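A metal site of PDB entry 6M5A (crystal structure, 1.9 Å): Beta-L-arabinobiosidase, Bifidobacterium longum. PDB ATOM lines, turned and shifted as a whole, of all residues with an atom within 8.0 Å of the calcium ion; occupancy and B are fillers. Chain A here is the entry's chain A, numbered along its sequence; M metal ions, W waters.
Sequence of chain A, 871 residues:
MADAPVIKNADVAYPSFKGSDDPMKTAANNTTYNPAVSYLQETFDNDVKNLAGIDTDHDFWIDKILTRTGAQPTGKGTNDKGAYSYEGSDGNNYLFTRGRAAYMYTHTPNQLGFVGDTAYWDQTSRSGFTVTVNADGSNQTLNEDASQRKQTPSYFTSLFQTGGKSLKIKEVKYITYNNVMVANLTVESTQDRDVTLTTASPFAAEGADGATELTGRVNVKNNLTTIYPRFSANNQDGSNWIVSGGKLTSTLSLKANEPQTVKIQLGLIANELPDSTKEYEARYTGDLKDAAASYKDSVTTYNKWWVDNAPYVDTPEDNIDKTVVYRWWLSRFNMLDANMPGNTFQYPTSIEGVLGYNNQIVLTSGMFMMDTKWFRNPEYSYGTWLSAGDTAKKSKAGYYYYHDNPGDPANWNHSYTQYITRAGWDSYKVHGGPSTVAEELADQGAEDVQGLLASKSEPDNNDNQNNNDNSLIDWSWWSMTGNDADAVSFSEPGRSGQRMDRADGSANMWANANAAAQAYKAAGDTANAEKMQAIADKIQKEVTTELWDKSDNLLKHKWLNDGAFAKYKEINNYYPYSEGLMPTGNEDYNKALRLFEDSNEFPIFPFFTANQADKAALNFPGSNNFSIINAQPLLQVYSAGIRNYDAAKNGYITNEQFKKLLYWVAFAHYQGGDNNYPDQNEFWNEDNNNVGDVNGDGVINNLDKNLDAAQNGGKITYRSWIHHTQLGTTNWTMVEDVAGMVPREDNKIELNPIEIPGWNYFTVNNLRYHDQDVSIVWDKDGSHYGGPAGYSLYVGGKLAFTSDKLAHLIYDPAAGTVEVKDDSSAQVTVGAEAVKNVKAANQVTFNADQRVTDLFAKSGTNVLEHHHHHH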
ATOM      1  N   MET A  24     -15.536  11.976   5.002  1.00  0.00           N
ATOM      2  CA  MET A  24     -14.566  12.942   5.583  1.00  0.00           C
ATOM      3  C   MET A  24     -14.900  14.381   5.133  1.00  0.00           C
ATOM      4  O   MET A  24     -14.130  15.261   5.459  1.00  0.00           O
ATOM      5  CB  MET A  24     -13.114  12.605   5.232  1.00  0.00           C
ATOM      6  CG  MET A  24     -12.575  11.424   6.023  1.00  0.00           C
ATOM      7  SD  MET A  24     -12.479  11.757   7.824  1.00  0.00           S
ATOM      8  CE  MET A  24     -11.226  13.029   7.866  1.00  0.00           C
ATOM      9  N   THR A  26     -14.564  16.092   2.519  1.00  0.00           N
ATOM     10  CA  THR A  26     -13.346  16.596   1.835  1.00  0.00           C
ATOM     11  C   THR A  26     -13.692  17.876   1.083  1.00  0.00           C
ATOM     12  O   THR A  26     -12.858  18.772   1.107  1.00  0.00           O
ATOM     13  CB  THR A  26     -12.697  15.573   0.901  1.00  0.00           C
ATOM     14  OG1 THR A  26     -13.648  15.215  -0.095  1.00  0.00           O
ATOM     15  CG2 THR A  26     -12.223  14.367   1.667  1.00  0.00           C
ATOM     16  N   TRP A  61     -14.823  21.921  10.547  1.00  0.00           N
ATOM     17  CA  TRP A  61     -14.691  20.676   9.762  1.00  0.00           C
ATOM     18  C   TRP A  61     -15.002  19.432  10.627  1.00  0.00           C
ATOM     19  O   TRP A  61     -15.722  18.542  10.141  1.00  0.00           O
ATOM     20  CB  TRP A  61     -13.313  20.621   9.145  1.00  0.00           C
ATOM     21  CG  TRP A  61     -13.154  19.566   8.131  1.00  0.00           C
ATOM     22  CD1 TRP A  61     -14.020  19.248   7.131  1.00  0.00           C
ATOM     23  CD2 TRP A  61     -12.052  18.666   8.028  1.00  0.00           C
ATOM     24  NE1 TRP A  61     -13.512  18.214   6.384  1.00  0.00           N
ATOM     25  CE2 TRP A  61     -12.298  17.854   6.895  1.00  0.00           C
ATOM     26  CE3 TRP A  61     -10.867  18.491   8.762  1.00  0.00           C
ATOM     27  CZ2 TRP A  61     -11.416  16.861   6.497  1.00  0.00           C
ATOM     28  CZ3 TRP A  61      -9.978  17.527   8.328  1.00  0.00           C
ATOM     29  CH2 TRP A  61     -10.237  16.738   7.206  1.00  0.00           C
ATOM     30  N   TYR A 312      -3.963  13.996  13.123  1.00  0.00           N
ATOM     31  CA  TYR A 312      -4.781  14.000  11.899  1.00  0.00           C
ATOM     32  C   TYR A 312      -4.350  12.813  11.032  1.00  0.00           C
ATOM     33  O   TYR A 312      -3.171  12.722  10.679  1.00  0.00           O
ATOM     34  CB  TYR A 312      -4.630  15.295  11.126  1.00  0.00           C
ATOM     35  CG  TYR A 312      -5.294  15.172   9.779  1.00  0.00           C
ATOM     36  CD1 TYR A 312      -6.672  15.043   9.687  1.00  0.00           C
ATOM     37  CD2 TYR A 312      -4.544  15.131   8.624  1.00  0.00           C
ATOM     38  CE1 TYR A 312      -7.289  14.917   8.453  1.00  0.00           C
ATOM     39  CE2 TYR A 312      -5.143  15.029   7.379  1.00  0.00           C
ATOM     40  CZ  TYR A 312      -6.515  14.901   7.309  1.00  0.00           C
ATOM     41  OH  TYR A 312      -7.091  14.775   6.088  1.00  0.00           O
ATOM     42  N   VAL A 313      -5.283  11.936  10.709  1.00  0.00           N
ATOM     43  CA  VAL A 313      -4.995  10.676   9.993  1.00  0.00           C
ATOM     44  C   VAL A 313      -5.696  10.732   8.649  1.00  0.00           C
ATOM     45  O   VAL A 313      -6.890  10.994   8.581  1.00  0.00           O
ATOM     46  CB  VAL A 313      -5.423   9.434  10.807  1.00  0.00           C
ATOM     47  CG1 VAL A 313      -5.373   8.178   9.970  1.00  0.00           C
ATOM     48  CG2 VAL A 313      -4.624   9.295  12.072  1.00  0.00           C
ATOM     49  N   ASP A 314      -4.949  10.431   7.593  1.00  0.00           N
ATOM     50  CA  ASP A 314      -5.548  10.427   6.236  1.00  0.00           C
ATOM     51  C   ASP A 314      -5.091   9.165   5.539  1.00  0.00           C
ATOM     52  O   ASP A 314      -3.863   8.944   5.434  1.00  0.00           O
ATOM     53  CB  ASP A 314      -5.150  11.689   5.456  1.00  0.00           C
ATOM     54  CG  ASP A 314      -5.676  11.714   4.034  1.00  0.00           C
ATOM     55  OD1 ASP A 314      -6.765  11.109   3.788  1.00  0.00           O
ATOM     56  OD2 ASP A 314      -4.999  12.354   3.188  1.00  0.00           O
ATOM     57  N   THR A 315      -6.036   8.347   5.099  1.00  0.00           N
ATOM     58  CA  THR A 315      -5.745   7.184   4.238  1.00  0.00           C
ATOM     59  C   THR A 315      -6.535   7.316   2.944  1.00  0.00           C
ATOM     60  O   THR A 315      -7.430   8.142   2.802  1.00  0.00           O
ATOM     61  CB  THR A 315      -6.071   5.856   4.932  1.00  0.00           C
ATOM     62  OG1 THR A 315      -7.495   5.710   4.857  1.00  0.00           O
ATOM     63  CG2 THR A 315      -5.619   5.767   6.380  1.00  0.00           C
ATOM     64  N   PRO A 316      -6.310   6.390   1.993  1.00  0.00           N
ATOM     65  CA  PRO A 316      -7.127   6.344   0.780  1.00  0.00           C
ATOM     66  C   PRO A 316      -8.570   5.913   1.036  1.00  0.00           C
ATOM     67  O   PRO A 316      -9.390   6.037   0.141  1.00  0.00           O
ATOM     68  CB  PRO A 316      -6.379   5.315  -0.081  1.00  0.00           C
ATOM     69  CG  PRO A 316      -4.988   5.341   0.457  1.00  0.00           C
ATOM     70  CD  PRO A 316      -5.176   5.456   1.963  1.00  0.00           C
ATOM     71  N   GLU A 317      -8.897   5.442   2.246  1.00  0.00           N
ATOM     72  CA  GLU A 317     -10.254   4.898   2.524  1.00  0.00           C
ATOM     73  C   GLU A 317     -10.933   5.834   3.531  1.00  0.00           C
ATOM     74  O   GLU A 317     -10.683   5.747   4.761  1.00  0.00           O
ATOM     75  CB  GLU A 317     -10.152   3.463   3.008  1.00  0.00           C
ATOM     76  CG  GLU A 317     -11.503   2.893   3.419  1.00  0.00           C
ATOM     77  CD  GLU A 317     -12.584   3.116   2.380  1.00  0.00           C
ATOM     78  OE1 GLU A 317     -12.492   2.426   1.370  1.00  0.00           O
ATOM     79  OE2 GLU A 317     -13.453   4.026   2.531  1.00  0.00           O
ATOM     80  N   ASP A 318     -11.784   6.705   3.038  1.00  0.00           N
ATOM     81  CA  ASP A 318     -12.329   7.803   3.864  1.00  0.00           C
ATOM     82  C   ASP A 318     -13.314   7.226   4.878  1.00  0.00           C
ATOM     83  O   ASP A 318     -13.557   7.918   5.893  1.00  0.00           O
ATOM     84  CB  ASP A 318     -12.912   8.905   2.988  1.00  0.00           C
ATOM     85  CG  ASP A 318     -11.842   9.794   2.373  1.00  0.00           C
ATOM     86  OD1 ASP A 318     -10.617   9.535   2.562  1.00  0.00           O
ATOM     87  OD2 ASP A 318     -12.250  10.755   1.678  1.00  0.00           O
ATOM     88  N   ASN A 319     -13.842   6.022   4.645  1.00  0.00           N
ATOM     89  CA  ASN A 319     -14.684   5.304   5.641  1.00  0.00           C
ATOM     90  C   ASN A 319     -13.853   4.984   6.881  1.00  0.00           C
ATOM     91  O   ASN A 319     -14.395   5.070   8.001  1.00  0.00           O
ATOM     92  CB  ASN A 319     -15.378   4.115   5.042  1.00  0.00           C
ATOM     93  CG  ASN A 319     -16.478   4.568   4.105  1.00  0.00           C
ATOM     94  OD1 ASN A 319     -17.492   5.082   4.578  1.00  0.00           O
ATOM     95  ND2 ASN A 319     -16.289   4.373   2.802  1.00  0.00           N
ATOM     96  N   ILE A 320     -12.594   4.598   6.701  1.00  0.00           N
ATOM     97  CA  ILE A 320     -11.702   4.316   7.859  1.00  0.00           C
ATOM     98  C   ILE A 320     -11.374   5.651   8.498  1.00  0.00           C
ATOM     99  O   ILE A 320     -11.492   5.792   9.741  1.00  0.00           O
ATOM    100  CB  ILE A 320     -10.455   3.555   7.422  1.00  0.00           C
ATOM    101  CG1 ILE A 320     -10.773   2.109   7.023  1.00  0.00           C
ATOM    102  CG2 ILE A 320      -9.428   3.601   8.532  1.00  0.00           C
ATOM    103  CD1 ILE A 320      -9.606   1.405   6.357  1.00  0.00           C
ATOM    104  N   ASP A 321     -11.033   6.636   7.678  1.00  0.00           N
ATOM    105  CA  ASP A 321     -10.652   7.975   8.207  1.00  0.00           C
ATOM    106  C   ASP A 321     -11.786   8.502   9.077  1.00  0.00           C
ATOM    107  O   ASP A 321     -11.535   9.040  10.128  1.00  0.00           O
ATOM    108  CB  ASP A 321     -10.350   8.920   7.062  1.00  0.00           C
ATOM    109  CG  ASP A 321      -9.145   8.498   6.256  1.00  0.00           C
ATOM    110  OD1 ASP A 321      -8.518   7.493   6.604  1.00  0.00           O
ATOM    111  OD2 ASP A 321      -8.829   9.250   5.345  1.00  0.00           O
ATOM    112  N   LYS A 322     -13.030   8.401   8.646  1.00  0.00           N
ATOM    113  CA  LYS A 322     -14.139   8.927   9.473  1.00  0.00           C
ATOM    114  C   LYS A 322     -14.241   8.126  10.791  1.00  0.00           C
ATOM    115  O   LYS A 322     -14.414   8.727  11.873  1.00  0.00           O
ATOM    116  CB  LYS A 322     -15.471   8.934   8.735  1.00  0.00           C
ATOM    117  CG  LYS A 322     -16.604   9.316   9.650  1.00  0.00           C
ATOM    118  CD  LYS A 322     -17.890   9.603   8.971  1.00  0.00           C
ATOM    119  CE  LYS A 322     -18.909  10.189   9.907  1.00  0.00           C
ATOM    120  NZ  LYS A 322     -20.156  10.452   9.174  1.00  0.00           N
ATOM    121  N   TYR A 761      -0.858   6.300  -0.813  1.00  0.00           N
ATOM    122  CA  TYR A 761      -0.591   7.436   0.093  1.00  0.00           C
ATOM    123  C   TYR A 761      -1.222   7.177   1.458  1.00  0.00           C
ATOM    124  O   TYR A 761      -2.158   6.402   1.595  1.00  0.00           O
ATOM    125  CB  TYR A 761      -1.105   8.754  -0.495  1.00  0.00           C
ATOM    126  CG  TYR A 761      -2.606   8.880  -0.567  1.00  0.00           C
ATOM    127  CD1 TYR A 761      -3.345   9.291   0.526  1.00  0.00           C
ATOM    128  CD2 TYR A 761      -3.304   8.500  -1.697  1.00  0.00           C
ATOM    129  CE1 TYR A 761      -4.722   9.395   0.481  1.00  0.00           C
ATOM    130  CE2 TYR A 761      -4.684   8.570  -1.750  1.00  0.00           C
ATOM    131  CZ  TYR A 761      -5.394   9.045  -0.662  1.00  0.00           C
ATOM    132  OH  TYR A 761      -6.755   9.115  -0.692  1.00  0.00           O
ATOM    133  N   PHE A 762      -0.707   7.916   2.436  1.00  0.00           N
ATOM    134  CA  PHE A 762      -1.382   8.155   3.723  1.00  0.00           C
ATOM    135  C   PHE A 762      -0.566   9.207   4.457  1.00  0.00           C
ATOM    136  O   PHE A 762       0.563   9.525   4.054  1.00  0.00           O
ATOM    137  CB  PHE A 762      -1.486   6.860   4.530  1.00  0.00           C
ATOM    138  CG  PHE A 762      -0.169   6.261   4.948  1.00  0.00           C
ATOM    139  CD1 PHE A 762       0.612   6.865   5.910  1.00  0.00           C
ATOM    140  CD2 PHE A 762       0.314   5.108   4.343  1.00  0.00           C
ATOM    141  CE1 PHE A 762       1.827   6.333   6.270  1.00  0.00           C
ATOM    142  CE2 PHE A 762       1.495   4.529   4.779  1.00  0.00           C
ATOM    143  CZ  PHE A 762       2.275   5.158   5.708  1.00  0.00           C
ATOM    144  N   THR A 763      -1.134   9.769   5.509  1.00  0.00           N
ATOM    145  CA  THR A 763      -0.371  10.636   6.437  1.00  0.00           C
ATOM    146  C   THR A 763      -0.937  10.530   7.833  1.00  0.00           C
ATOM    147  O   THR A 763      -2.186  10.317   8.028  1.00  0.00           O
ATOM    148  CB  THR A 763      -0.314  12.101   5.968  1.00  0.00           C
ATOM    149  OG1 THR A 763       0.692  12.682   6.785  1.00  0.00           O
ATOM    150  CG2 THR A 763      -1.630  12.837   6.105  1.00  0.00           C
ATOM    151  N   HIS A 784       0.087  12.586  -4.823  1.00  0.00           N
ATOM    152  CA  HIS A 784      -1.113  12.822  -3.975  1.00  0.00           C
ATOM    153  C   HIS A 784      -1.008  14.143  -3.184  1.00  0.00           C
ATOM    154  O   HIS A 784      -1.994  14.859  -3.168  1.00  0.00           O
ATOM    155  CB  HIS A 784      -1.422  11.632  -3.059  1.00  0.00           C
ATOM    156  CG  HIS A 784      -2.683  11.868  -2.334  1.00  0.00           C
ATOM    157  ND1 HIS A 784      -3.906  11.846  -2.978  1.00  0.00           N
ATOM    158  CD2 HIS A 784      -2.928  12.239  -1.059  1.00  0.00           C
ATOM    159  CE1 HIS A 784      -4.864  12.152  -2.119  1.00  0.00           C
ATOM    160  NE2 HIS A 784      -4.274  12.388  -0.927  1.00  0.00           N
ATOM    161  N   TYR A 785       0.111  14.420  -2.497  1.00  0.00           N
ATOM    162  CA  TYR A 785       0.268  15.585  -1.598  1.00  0.00           C
ATOM    163  C   TYR A 785       1.141  16.662  -2.264  1.00  0.00           C
ATOM    164  O   TYR A 785       1.165  17.786  -1.759  1.00  0.00           O
ATOM    165  CB  TYR A 785       0.839  15.144  -0.246  1.00  0.00           C
ATOM    166  CG  TYR A 785      -0.057  14.253   0.575  1.00  0.00           C
ATOM    167  CD1 TYR A 785      -1.313  14.651   0.971  1.00  0.00           C
ATOM    168  CD2 TYR A 785       0.381  13.006   0.984  1.00  0.00           C
ATOM    169  CE1 TYR A 785      -2.110  13.864   1.781  1.00  0.00           C
ATOM    170  CE2 TYR A 785      -0.412  12.191   1.785  1.00  0.00           C
ATOM    171  CZ  TYR A 785      -1.664  12.619   2.178  1.00  0.00           C
ATOM    172  OH  TYR A 785      -2.433  11.795   2.950  1.00  0.00           O
HETATM  173 CA    CA M   1      -8.584  10.078   3.193  1.00  0.00          CA
HETATM  174  O   HOH W   1      -9.629  12.076   3.637  1.00  0.00           O
HETATM  175  O   HOH W   2      -8.109  10.704   1.000  1.00  0.00           O
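The nearest printed residue that does not touch the calcium ion is Tyr 761 (4.4 Å).
The calcium ion is bound by OD1 of Asp 314, at 2.2 Å.
The side-chain carboxylate (OD1) of Asp 318 is bound to the calcium ion, at 2.2 Å.
The calcium ion is bound by the backbone carbonyl oxygen (O) of Thr 315 (2.3 Å).
Water W1 is bound to the calcium ion (2.3 Å).
OD2 of Asp 321 binds the calcium ion.
The calcium ion is bound by water W2, at 2.3 Å.
The backbone NH (N) of Glu 317 sits at hydrogen-bond distance from the side-chain hydroxyl (OG1) of Thr 315 (3.0 Å).
The backbone NH of Asp 314 is in hydrogen-bond range of the backbone carbonyl oxygen of Thr 763 (2.8 Å).
OD2 of Asp 314 is in hydrogen-bond range of OH of Tyr 785.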
